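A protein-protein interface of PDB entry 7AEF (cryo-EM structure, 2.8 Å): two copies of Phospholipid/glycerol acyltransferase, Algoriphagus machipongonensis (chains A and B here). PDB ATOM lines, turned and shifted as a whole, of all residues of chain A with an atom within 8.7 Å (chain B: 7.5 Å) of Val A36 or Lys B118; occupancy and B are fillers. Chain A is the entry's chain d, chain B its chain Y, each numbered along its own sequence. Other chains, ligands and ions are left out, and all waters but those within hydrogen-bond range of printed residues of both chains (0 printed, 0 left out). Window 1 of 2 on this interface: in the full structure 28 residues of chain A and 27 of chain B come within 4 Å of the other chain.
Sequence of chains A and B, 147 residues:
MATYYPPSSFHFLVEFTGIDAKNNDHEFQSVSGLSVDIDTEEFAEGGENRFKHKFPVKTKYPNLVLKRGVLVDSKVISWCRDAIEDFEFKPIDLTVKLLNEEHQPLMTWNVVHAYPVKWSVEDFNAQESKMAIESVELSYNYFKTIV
Of the printed residues of chain B, Val A36 touches Lys B118 (3.7 Å) and Trp B119 (3.2 Å). Lys B118 touches just these residues of chain A: Val A36 (3.7 Å) and Asp A37 (3.1 Å). Of the printed residues of chain B, Thr A59 touches Ile B84 (3.3 Å). Of the printed residues of chain B, Asp A37 touches Val B117 (3.6 Å) and Lys B118 (3.1 Å). Printed residues of chain B within 4 Å of Ser A35: Trp B119 (3.8 Å) and Ser B120 (3.3 Å). Of the printed residues of chain A, Ile B84 touches Thr A59 (3.3 Å). Printed residues of chain A within 4 Å of Ser B120: Ser A35. The nearest printed residue of chain B that does not touch Ile A38 is Ile B84 (4.6 Å).
O of Leu A34 touches N of Val B121, 3.9 Å away. CA of Ser A35 touches O of Trp B119, at 3.8 Å. CB of Ser B120 touches CB of Ser A35 (3.3 Å). Val A36 touches Lys B118 (O to CG, 3.7 Å). Asp A37 touches Val B117 (CA to O, 3.6 Å). Ile A38 touches Pro B116.
The backbone carbonyl oxygen (O) of Trp B119 lies within hydrogen-bond range of the backbone NH (N) of Val A36 (3.2 Å). The side-chain carboxylate (OD1) of Asp A37 is in salt-bridge range of the side-chain amino group (NZ) of Lys B118, 3.6 Å away. O of Val B117 sits at hydrogen-bond distance from N of Ile A38, 3.1 Å away. O of Ile B84 is in hydrogen-bond range of OG1 of Thr A59, at 3.3 Å.
Along chain B the printed residues that touch a printed residue of chain A span positions 84 to 121. Of the 17 printed residues of chain A, 6 touch a printed residue of chain B. Along chain A the printed residues that touch a printed residue of chain B span positions 34 to 59. Among the printed residues, Asp or Glu carboxylates within 4 Å of a Lys or Arg side-chain nitrogen of the other chain: Asp A37 with Lys B118.
O of Ser B120 lies within hydrogen-bond range of N of Ser B135, at 2.9 Å. The backbone carbonyl oxygen (O) of Asp A37 lies within hydrogen-bond range of the backbone NH (N) of Lys A60, 2.8 Å away. The backbone carbonyl oxygen (O) of Glu B137 is in hydrogen-bond range of the backbone NH (N) of Val B117, at 3.0 Å. N of Glu B137 sits at hydrogen-bond distance from O of Lys B118.
No position is printed for both chains. Of the 10 pairs that touch across the chains among the printed residues, none has its exchanged pair printed and touching as well.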
ATOM      1  N   GLY A  33      26.050 -22.951   6.557  1.00  0.00           N
ATOM      2  CA  GLY A  33      26.609 -21.608   6.523  1.00  0.00           C
ATOM      3  C   GLY A  33      26.807 -21.013   5.134  1.00  0.00           C
ATOM      4  O   GLY A  33      27.351 -19.914   5.011  1.00  0.00           O
ATOM      5  N   LEU A  34      26.349 -21.676   4.083  1.00  0.00           N
ATOM      6  CA  LEU A  34      26.535 -21.145   2.733  1.00  0.00           C
ATOM      7  C   LEU A  34      25.453 -20.126   2.367  1.00  0.00           C
ATOM      8  O   LEU A  34      24.562 -20.393   1.559  1.00  0.00           O
ATOM      9  CB  LEU A  34      26.555 -22.284   1.724  1.00  0.00           C
ATOM     10  CG  LEU A  34      27.697 -23.300   1.835  1.00  0.00           C
ATOM     11  CD1 LEU A  34      27.461 -24.415   0.861  1.00  0.00           C
ATOM     12  CD2 LEU A  34      29.050 -22.640   1.558  1.00  0.00           C
ATOM     13  N   SER A  35      25.564 -18.917   2.944  1.00  0.00           N
ATOM     14  CA  SER A  35      24.576 -17.881   2.648  1.00  0.00           C
ATOM     15  C   SER A  35      25.258 -16.502   2.716  1.00  0.00           C
ATOM     16  O   SER A  35      26.430 -16.393   3.080  1.00  0.00           O
ATOM     17  CB  SER A  35      23.420 -17.849   3.639  1.00  0.00           C
ATOM     18  OG  SER A  35      23.847 -17.639   4.955  1.00  0.00           O
ATOM     19  N   VAL A  36      24.493 -15.436   2.414  1.00  0.00           N
ATOM     20  CA  VAL A  36      24.991 -14.048   2.449  1.00  0.00           C
ATOM     21  C   VAL A  36      23.896 -13.006   2.650  1.00  0.00           C
ATOM     22  O   VAL A  36      22.745 -13.289   2.346  1.00  0.00           O
ATOM     23  CB  VAL A  36      25.746 -13.694   1.152  1.00  0.00           C
ATOM     24  CG1 VAL A  36      24.867 -13.930  -0.064  1.00  0.00           C
ATOM     25  CG2 VAL A  36      26.245 -12.272   1.168  1.00  0.00           C
ATOM     26  N   ASP A  37      24.236 -11.796   3.165  1.00  0.00           N
ATOM     27  CA  ASP A  37      23.312 -10.692   3.381  1.00  0.00           C
ATOM     28  C   ASP A  37      23.938  -9.301   3.179  1.00  0.00           C
ATOM     29  O   ASP A  37      25.156  -9.141   3.218  1.00  0.00           O
ATOM     30  CB  ASP A  37      22.711 -10.776   4.783  1.00  0.00           C
ATOM     31  CG  ASP A  37      21.952 -12.068   5.037  1.00  0.00           C
ATOM     32  OD1 ASP A  37      21.481 -12.299   6.142  1.00  0.00           O
ATOM     33  OD2 ASP A  37      21.800 -12.913   4.265  1.00  0.00           O
ATOM     34  N   ILE A  38      23.106  -8.271   2.998  1.00  0.00           N
ATOM     35  CA  ILE A  38      23.636  -6.918   2.825  1.00  0.00           C
ATOM     36  C   ILE A  38      23.148  -5.980   3.924  1.00  0.00           C
ATOM     37  O   ILE A  38      21.941  -5.771   4.078  1.00  0.00           O
ATOM     38  CB  ILE A  38      23.283  -6.341   1.449  1.00  0.00           C
ATOM     39  CG1 ILE A  38      23.783  -7.262   0.338  1.00  0.00           C
ATOM     40  CG2 ILE A  38      23.877  -4.949   1.299  1.00  0.00           C
ATOM     41  CD1 ILE A  38      23.466  -6.770  -1.051  1.00  0.00           C
ATOM     42  N   ASP A  39      24.093  -5.398   4.662  1.00  0.00           N
ATOM     43  CA  ASP A  39      23.765  -4.392   5.664  1.00  0.00           C
ATOM     44  C   ASP A  39      23.298  -3.132   4.977  1.00  0.00           C
ATOM     45  O   ASP A  39      23.935  -2.680   4.023  1.00  0.00           O
ATOM     46  CB  ASP A  39      24.968  -3.983   6.517  1.00  0.00           C
ATOM     47  CG  ASP A  39      25.400  -5.005   7.526  1.00  0.00           C
ATOM     48  OD1 ASP A  39      24.676  -5.945   7.835  1.00  0.00           O
ATOM     49  OD2 ASP A  39      26.484  -4.811   8.084  1.00  0.00           O
ATOM     50  N   THR A  40      22.257  -2.508   5.535  1.00  0.00           N
ATOM     51  CA  THR A  40      21.699  -1.264   5.030  1.00  0.00           C
ATOM     52  C   THR A  40      21.535  -0.190   6.107  1.00  0.00           C
ATOM     53  O   THR A  40      21.538  -0.473   7.300  1.00  0.00           O
ATOM     54  CB  THR A  40      20.321  -1.472   4.386  1.00  0.00           C
ATOM     55  OG1 THR A  40      19.397  -1.875   5.393  1.00  0.00           O
ATOM     56  CG2 THR A  40      20.364  -2.513   3.282  1.00  0.00           C
ATOM     57  N   LYS A  58      27.353  -2.879   3.276  1.00  0.00           N
ATOM     58  CA  LYS A  58      28.330  -3.981   3.222  1.00  0.00           C
ATOM     59  C   LYS A  58      27.718  -5.358   2.980  1.00  0.00           C
ATOM     60  O   LYS A  58      26.628  -5.671   3.455  1.00  0.00           O
ATOM     61  CB  LYS A  58      29.137  -4.151   4.516  1.00  0.00           C
ATOM     62  CG  LYS A  58      30.153  -3.105   4.861  1.00  0.00           C
ATOM     63  CD  LYS A  58      31.402  -3.209   4.024  1.00  0.00           C
ATOM     64  CE  LYS A  58      32.428  -2.198   4.489  1.00  0.00           C
ATOM     65  NZ  LYS A  58      33.627  -2.183   3.628  1.00  0.00           N
ATOM     66  N   THR A  59      28.491  -6.218   2.324  1.00  0.00           N
ATOM     67  CA  THR A  59      28.120  -7.615   2.159  1.00  0.00           C
ATOM     68  C   THR A  59      28.669  -8.429   3.325  1.00  0.00           C
ATOM     69  O   THR A  59      29.827  -8.271   3.707  1.00  0.00           O
ATOM     70  CB  THR A  59      28.653  -8.164   0.833  1.00  0.00           C
ATOM     71  OG1 THR A  59      28.099  -7.421  -0.250  1.00  0.00           O
ATOM     72  CG2 THR A  59      28.262  -9.560   0.652  1.00  0.00           C
ATOM     73  N   LYS A  60      27.844  -9.318   3.873  1.00  0.00           N
ATOM     74  CA  LYS A  60      28.161 -10.069   5.076  1.00  0.00           C
ATOM     75  C   LYS A  60      28.004 -11.583   4.898  1.00  0.00           C
ATOM     76  O   LYS A  60      27.026 -12.034   4.317  1.00  0.00           O
ATOM     77  CB  LYS A  60      27.227  -9.557   6.133  1.00  0.00           C
ATOM     78  CG  LYS A  60      27.545  -9.923   7.530  1.00  0.00           C
ATOM     79  CD  LYS A  60      26.449  -9.387   8.424  1.00  0.00           C
ATOM     80  CE  LYS A  60      26.625  -9.869   9.845  1.00  0.00           C
ATOM     81  NZ  LYS A  60      25.686  -9.174  10.754  1.00  0.00           N
ATOM     82  N   TYR A  61      28.946 -12.377   5.416  1.00  0.00           N
ATOM     83  CA  TYR A  61      28.886 -13.837   5.355  1.00  0.00           C
ATOM     84  C   TYR A  61      29.007 -14.446   6.754  1.00  0.00           C
ATOM     85  O   TYR A  61      29.752 -13.922   7.574  1.00  0.00           O
ATOM     86  CB  TYR A  61      30.020 -14.379   4.476  1.00  0.00           C
ATOM     87  CG  TYR A  61      30.015 -13.955   3.036  1.00  0.00           C
ATOM     88  CD1 TYR A  61      30.593 -12.766   2.639  1.00  0.00           C
ATOM     89  CD2 TYR A  61      29.476 -14.773   2.077  1.00  0.00           C
ATOM     90  CE1 TYR A  61      30.596 -12.402   1.332  1.00  0.00           C
ATOM     91  CE2 TYR A  61      29.486 -14.419   0.768  1.00  0.00           C
ATOM     92  CZ  TYR A  61      30.043 -13.237   0.401  1.00  0.00           C
ATOM     93  OH  TYR A  61      30.040 -12.880  -0.917  1.00  0.00           O
ATOM     94  N   PRO A  62      28.265 -15.523   7.042  1.00  0.00           N
ATOM     95  CA  PRO A  62      28.377 -16.306   8.286  1.00  0.00           C
ATOM     96  C   PRO A  62      29.510 -17.319   8.214  1.00  0.00           C
ATOM     97  O   PRO A  62      29.961 -17.670   7.128  1.00  0.00           O
ATOM     98  CB  PRO A  62      27.033 -17.045   8.311  1.00  0.00           C
ATOM     99  CG  PRO A  62      26.732 -17.237   6.877  1.00  0.00           C
ATOM    100  CD  PRO A  62      27.217 -16.024   6.170  1.00  0.00           C
ATOM    101  N   TYR A 140      35.849 -17.185   6.877  1.00  0.00           N
ATOM    102  CA  TYR A 140      36.337 -17.038   5.498  1.00  0.00           C
ATOM    103  C   TYR A 140      35.952 -15.649   4.997  1.00  0.00           C
ATOM    104  O   TYR A 140      35.188 -14.945   5.647  1.00  0.00           O
ATOM    105  CB  TYR A 140      35.807 -18.157   4.578  1.00  0.00           C
ATOM    106  CG  TYR A 140      34.334 -18.161   4.482  1.00  0.00           C
ATOM    107  CD1 TYR A 140      33.684 -17.495   3.461  1.00  0.00           C
ATOM    108  CD2 TYR A 140      33.586 -18.816   5.427  1.00  0.00           C
ATOM    109  CE1 TYR A 140      32.334 -17.462   3.409  1.00  0.00           C
ATOM    110  CE2 TYR A 140      32.259 -18.792   5.382  1.00  0.00           C
ATOM    111  CZ  TYR A 140      31.623 -18.117   4.383  1.00  0.00           C
ATOM    112  OH  TYR A 140      30.262 -18.097   4.391  1.00  0.00           O
ATOM    113  N   ASN A 141      36.480 -15.242   3.837  1.00  0.00           N
ATOM    114  CA  ASN A 141      36.197 -13.887   3.355  1.00  0.00           C
ATOM    115  C   ASN A 141      34.946 -13.788   2.496  1.00  0.00           C
ATOM    116  O   ASN A 141      34.148 -12.866   2.670  1.00  0.00           O
ATOM    117  CB  ASN A 141      37.368 -13.340   2.557  1.00  0.00           C
ATOM    118  CG  ASN A 141      38.521 -12.952   3.414  1.00  0.00           C
ATOM    119  OD1 ASN A 141      38.397 -12.699   4.604  1.00  0.00           O
ATOM    120  ND2 ASN A 141      39.664 -12.891   2.805  1.00  0.00           N
ATOM    121  N   TYR A 142      34.801 -14.688   1.536  1.00  0.00           N
ATOM    122  CA  TYR A 142      33.664 -14.681   0.632  1.00  0.00           C
ATOM    123  C   TYR A 142      33.613 -16.013  -0.082  1.00  0.00           C
ATOM    124  O   TYR A 142      34.510 -16.846   0.052  1.00  0.00           O
ATOM    125  CB  TYR A 142      33.731 -13.543  -0.387  1.00  0.00           C
ATOM    126  CG  TYR A 142      34.896 -13.567  -1.315  1.00  0.00           C
ATOM    127  CD1 TYR A 142      34.824 -14.222  -2.531  1.00  0.00           C
ATOM    128  CD2 TYR A 142      36.055 -12.904  -0.993  1.00  0.00           C
ATOM    129  CE1 TYR A 142      35.868 -14.235  -3.373  1.00  0.00           C
ATOM    130  CE2 TYR A 142      37.108 -12.902  -1.841  1.00  0.00           C
ATOM    131  CZ  TYR A 142      37.013 -13.570  -3.032  1.00  0.00           C
ATOM    132  OH  TYR A 142      38.066 -13.580  -3.900  1.00  0.00           O
ATOM    133  N   PHE A 143      32.559 -16.190  -0.864  1.00  0.00           N
ATOM    134  CA  PHE A 143      32.493 -17.333  -1.744  1.00  0.00           C
ATOM    135  C   PHE A 143      31.918 -16.952  -3.093  1.00  0.00           C
ATOM    136  O   PHE A 143      31.188 -15.975  -3.228  1.00  0.00           O
ATOM    137  CB  PHE A 143      31.718 -18.524  -1.133  1.00  0.00           C
ATOM    138  CG  PHE A 143      30.248 -18.312  -0.915  1.00  0.00           C
ATOM    139  CD1 PHE A 143      29.336 -18.500  -1.928  1.00  0.00           C
ATOM    140  CD2 PHE A 143      29.769 -18.029   0.339  1.00  0.00           C
ATOM    141  CE1 PHE A 143      28.004 -18.336  -1.710  1.00  0.00           C
ATOM    142  CE2 PHE A 143      28.420 -17.880   0.558  1.00  0.00           C
ATOM    143  CZ  PHE A 143      27.545 -18.027  -0.463  1.00  0.00           C
ATOM    144  N   ASN B  63      10.260  -6.540   3.992  1.00  0.00           N
ATOM    145  CA  ASN B  63      10.838  -7.150   2.794  1.00  0.00           C
ATOM    146  C   ASN B  63       9.969  -8.280   2.254  1.00  0.00           C
ATOM    147  O   ASN B  63       9.215  -8.918   2.986  1.00  0.00           O
ATOM    148  CB  ASN B  63      12.223  -7.710   3.065  1.00  0.00           C
ATOM    149  CG  ASN B  63      13.249  -6.651   3.307  1.00  0.00           C
ATOM    150  OD1 ASN B  63      13.115  -5.485   2.942  1.00  0.00           O
ATOM    151  ND2 ASN B  63      14.310  -7.066   3.932  1.00  0.00           N
ATOM    152  N   VAL B  65       9.647 -11.963   0.626  1.00  0.00           N
ATOM    153  CA  VAL B  65      10.403 -13.209   0.710  1.00  0.00           C
ATOM    154  C   VAL B  65       9.825 -14.294  -0.193  1.00  0.00           C
ATOM    155  O   VAL B  65       8.637 -14.621  -0.108  1.00  0.00           O
ATOM    156  CB  VAL B  65      10.488 -13.705   2.160  1.00  0.00           C
ATOM    157  CG1 VAL B  65      11.229 -15.028   2.231  1.00  0.00           C
ATOM    158  CG2 VAL B  65      11.195 -12.672   2.993  1.00  0.00           C
ATOM    159  N   ILE B  77      18.651 -15.283 -10.098  1.00  0.00           N
ATOM    160  CA  ILE B  77      19.857 -15.408  -9.300  1.00  0.00           C
ATOM    161  C   ILE B  77      21.028 -14.692  -9.959  1.00  0.00           C
ATOM    162  O   ILE B  77      21.794 -14.030  -9.253  1.00  0.00           O
ATOM    163  CB  ILE B  77      20.196 -16.870  -8.970  1.00  0.00           C
ATOM    164  CG1 ILE B  77      19.066 -17.517  -8.134  1.00  0.00           C
ATOM    165  CG2 ILE B  77      21.517 -16.923  -8.193  1.00  0.00           C
ATOM    166  CD1 ILE B  77      18.720 -16.856  -6.791  1.00  0.00           C
ATOM    167  N   CYS B  80      20.713 -11.269  -8.868  1.00  0.00           N
ATOM    168  CA  CYS B  80      21.091 -11.139  -7.467  1.00  0.00           C
ATOM    169  C   CYS B  80      22.601 -11.117  -7.301  1.00  0.00           C
ATOM    170  O   CYS B  80      23.127 -10.288  -6.554  1.00  0.00           O
ATOM    171  CB  CYS B  80      20.518 -12.294  -6.656  1.00  0.00           C
ATOM    172  SG  CYS B  80      18.751 -12.279  -6.487  1.00  0.00           S
ATOM    173  N   ILE B  84      25.146  -8.573  -5.310  1.00  0.00           N
ATOM    174  CA  ILE B  84      25.834  -9.137  -4.143  1.00  0.00           C
ATOM    175  C   ILE B  84      27.348  -9.046  -4.274  1.00  0.00           C
ATOM    176  O   ILE B  84      28.049  -8.697  -3.314  1.00  0.00           O
ATOM    177  CB  ILE B  84      25.414 -10.600  -3.931  1.00  0.00           C
ATOM    178  CG1 ILE B  84      23.956 -10.671  -3.465  1.00  0.00           C
ATOM    179  CG2 ILE B  84      26.356 -11.304  -2.932  1.00  0.00           C
ATOM    180  CD1 ILE B  84      23.327 -12.063  -3.534  1.00  0.00           C
ATOM    181  N   GLU B  85      27.878  -9.422  -5.429  1.00  0.00           N
ATOM    182  CA  GLU B  85      29.316  -9.493  -5.628  1.00  0.00           C
ATOM    183  C   GLU B  85      29.952  -8.174  -6.066  1.00  0.00           C
ATOM    184  O   GLU B  85      31.060  -7.864  -5.619  1.00  0.00           O
ATOM    185  CB  GLU B  85      29.627 -10.596  -6.638  1.00  0.00           C
ATOM    186  CG  GLU B  85      29.292 -11.994  -6.112  1.00  0.00           C
ATOM    187  CD  GLU B  85      29.510 -13.096  -7.120  1.00  0.00           C
ATOM    188  OE1 GLU B  85      29.781 -12.797  -8.281  1.00  0.00           O
ATOM    189  OE2 GLU B  85      29.397 -14.266  -6.753  1.00  0.00           O
ATOM    190  N   TYR B 115      14.998  -4.562  -5.081  1.00  0.00           N
ATOM    191  CA  TYR B 115      16.355  -5.044  -5.329  1.00  0.00           C
ATOM    192  C   TYR B 115      16.771  -6.080  -4.265  1.00  0.00           C
ATOM    193  O   TYR B 115      16.190  -6.131  -3.179  1.00  0.00           O
ATOM    194  CB  TYR B 115      17.310  -3.836  -5.431  1.00  0.00           C
ATOM    195  CG  TYR B 115      17.621  -3.149  -4.184  1.00  0.00           C
ATOM    196  CD1 TYR B 115      18.676  -3.546  -3.398  1.00  0.00           C
ATOM    197  CD2 TYR B 115      16.882  -2.066  -3.805  1.00  0.00           C
ATOM    198  CE1 TYR B 115      18.971  -2.896  -2.250  1.00  0.00           C
ATOM    199  CE2 TYR B 115      17.175  -1.396  -2.660  1.00  0.00           C
ATOM    200  CZ  TYR B 115      18.223  -1.814  -1.884  1.00  0.00           C
ATOM    201  OH  TYR B 115      18.535  -1.147  -0.731  1.00  0.00           O
ATOM    202  N   PRO B 116      17.778  -6.922  -4.555  1.00  0.00           N
ATOM    203  CA  PRO B 116      18.127  -8.034  -3.644  1.00  0.00           C
ATOM    204  C   PRO B 116      18.928  -7.654  -2.407  1.00  0.00           C
ATOM    205  O   PRO B 116      19.904  -6.923  -2.500  1.00  0.00           O
ATOM    206  CB  PRO B 116      18.961  -8.955  -4.531  1.00  0.00           C
ATOM    207  CG  PRO B 116      19.256  -8.202  -5.775  1.00  0.00           C
ATOM    208  CD  PRO B 116      18.750  -6.848  -5.658  1.00  0.00           C
ATOM    209  N   VAL B 117      18.522  -8.167  -1.248  1.00  0.00           N
ATOM    210  CA  VAL B 117      19.286  -7.977  -0.021  1.00  0.00           C
ATOM    211  C   VAL B 117      19.733  -9.286   0.596  1.00  0.00           C
ATOM    212  O   VAL B 117      20.593  -9.268   1.476  1.00  0.00           O
ATOM    213  CB  VAL B 117      18.554  -7.117   1.047  1.00  0.00           C
ATOM    214  CG1 VAL B 117      18.575  -5.643   0.704  1.00  0.00           C
ATOM    215  CG2 VAL B 117      17.153  -7.615   1.380  1.00  0.00           C
ATOM    216  N   LYS B 118      19.206 -10.422   0.167  1.00  0.00           N
ATOM    217  CA  LYS B 118      19.594 -11.679   0.786  1.00  0.00           C
ATOM    218  C   LYS B 118      19.443 -12.883  -0.143  1.00  0.00           C
ATOM    219  O   LYS B 118      18.554 -12.915  -0.975  1.00  0.00           O
ATOM    220  CB  LYS B 118      18.750 -11.868   2.028  1.00  0.00           C
ATOM    221  CG  LYS B 118      19.076 -13.078   2.835  1.00  0.00           C
ATOM    222  CD  LYS B 118      18.494 -12.948   4.198  1.00  0.00           C
ATOM    223  CE  LYS B 118      18.696 -14.226   4.964  1.00  0.00           C
ATOM    224  NZ  LYS B 118      18.342 -14.044   6.390  1.00  0.00           N
ATOM    225  N   TRP B 119      20.312 -13.883   0.009  1.00  0.00           N
ATOM    226  CA  TRP B 119      20.229 -15.131  -0.742  1.00  0.00           C
ATOM    227  C   TRP B 119      20.820 -16.269   0.072  1.00  0.00           C
ATOM    228  O   TRP B 119      21.952 -16.157   0.545  1.00  0.00           O
ATOM    229  CB  TRP B 119      20.980 -15.021  -2.064  1.00  0.00           C
ATOM    230  CG  TRP B 119      21.024 -16.292  -2.866  1.00  0.00           C
ATOM    231  CD1 TRP B 119      20.016 -17.191  -3.071  1.00  0.00           C
ATOM    232  CD2 TRP B 119      22.147 -16.794  -3.572  1.00  0.00           C
ATOM    233  NE1 TRP B 119      20.452 -18.214  -3.858  1.00  0.00           N
ATOM    234  CE2 TRP B 119      21.760 -17.994  -4.176  1.00  0.00           C
ATOM    235  CE3 TRP B 119      23.451 -16.343  -3.754  1.00  0.00           C
ATOM    236  CZ2 TRP B 119      22.621 -18.744  -4.939  1.00  0.00           C
ATOM    237  CZ3 TRP B 119      24.309 -17.092  -4.517  1.00  0.00           C
ATOM    238  CH2 TRP B 119      23.894 -18.274  -5.100  1.00  0.00           C
ATOM    239  N   SER B 120      20.082 -17.372   0.205  1.00  0.00           N
ATOM    240  CA  SER B 120      20.606 -18.507   0.958  1.00  0.00           C
ATOM    241  C   SER B 120      20.044 -19.855   0.516  1.00  0.00           C
ATOM    242  O   SER B 120      19.026 -19.946  -0.178  1.00  0.00           O
ATOM    243  CB  SER B 120      20.340 -18.334   2.443  1.00  0.00           C
ATOM    244  OG  SER B 120      18.961 -18.367   2.717  1.00  0.00           O
ATOM    245  N   VAL B 121      20.751 -20.921   0.932  1.00  0.00           N
ATOM    246  CA  VAL B 121      20.317 -22.288   0.665  1.00  0.00           C
ATOM    247  C   VAL B 121      20.403 -23.034   1.997  1.00  0.00           C
ATOM    248  O   VAL B 121      21.372 -22.869   2.746  1.00  0.00           O
ATOM    249  CB  VAL B 121      21.185 -22.975  -0.415  1.00  0.00           C
ATOM    250  CG1 VAL B 121      20.843 -24.464  -0.545  1.00  0.00           C
ATOM    251  CG2 VAL B 121      21.073 -22.255  -1.728  1.00  0.00           C
ATOM    252  N   SER B 135      16.224 -19.663  -0.961  1.00  0.00           N
ATOM    253  CA  SER B 135      15.465 -18.521  -0.468  1.00  0.00           C
ATOM    254  C   SER B 135      16.057 -17.163  -0.850  1.00  0.00           C
ATOM    255  O   SER B 135      17.260 -16.923  -0.703  1.00  0.00           O
ATOM    256  CB  SER B 135      15.337 -18.616   1.042  1.00  0.00           C
ATOM    257  OG  SER B 135      14.731 -17.456   1.543  1.00  0.00           O
ATOM    258  N   VAL B 136      15.192 -16.277  -1.360  1.00  0.00           N
ATOM    259  CA  VAL B 136      15.568 -14.939  -1.832  1.00  0.00           C
ATOM    260  C   VAL B 136      14.710 -13.845  -1.191  1.00  0.00           C
ATOM    261  O   VAL B 136      13.477 -13.908  -1.208  1.00  0.00           O
ATOM    262  CB  VAL B 136      15.477 -14.849  -3.367  1.00  0.00           C
ATOM    263  CG1 VAL B 136      15.784 -13.445  -3.859  1.00  0.00           C
ATOM    264  CG2 VAL B 136      16.461 -15.812  -3.981  1.00  0.00           C
ATOM    265  N   GLU B 137      15.363 -12.807  -0.676  1.00  0.00           N
ATOM    266  CA  GLU B 137      14.668 -11.691  -0.054  1.00  0.00           C
ATOM    267  C   GLU B 137      14.971 -10.366  -0.751  1.00  0.00           C
ATOM    268  O   GLU B 137      16.135 -10.049  -1.017  1.00  0.00           O
ATOM    269  CB  GLU B 137      15.032 -11.658   1.419  1.00  0.00           C
ATOM    270  CG  GLU B 137      14.406 -10.595   2.227  1.00  0.00           C
ATOM    271  CD  GLU B 137      14.661 -10.838   3.678  1.00  0.00           C
ATOM    272  OE1 GLU B 137      15.071 -11.951   4.006  1.00  0.00           O
ATOM    273  OE2 GLU B 137      14.518  -9.918   4.489  1.00  0.00           O
ATOM    274  N   LEU B 138      13.907  -9.597  -1.042  1.00  0.00           N
ATOM    275  CA  LEU B 138      13.989  -8.319  -1.759  1.00  0.00           C
ATOM    276  C   LEU B 138      13.473  -7.105  -0.981  1.00  0.00           C
ATOM    277  O   LEU B 138      12.426  -7.157  -0.329  1.00  0.00           O
ATOM    278  CB  LEU B 138      13.197  -8.375  -3.062  1.00  0.00           C
ATOM    279  CG  LEU B 138      13.492  -9.492  -4.058  1.00  0.00           C
ATOM    280  CD1 LEU B 138      12.546  -9.385  -5.221  1.00  0.00           C
ATOM    281  CD2 LEU B 138      14.907  -9.423  -4.521  1.00  0.00           C
ATOM    282  N   SER B 139      14.150  -5.968  -1.153  1.00  0.00           N
ATOM    283  CA  SER B 139      13.712  -4.720  -0.545  1.00  0.00           C
ATOM    284  C   SER B 139      12.961  -3.955  -1.632  1.00  0.00           C
ATOM    285  O   SER B 139      13.311  -4.081  -2.791  1.00  0.00           O
ATOM    286  CB  SER B 139      14.903  -3.900  -0.063  1.00  0.00           C
ATOM    287  OG  SER B 139      14.521  -2.579   0.201  1.00  0.00           O
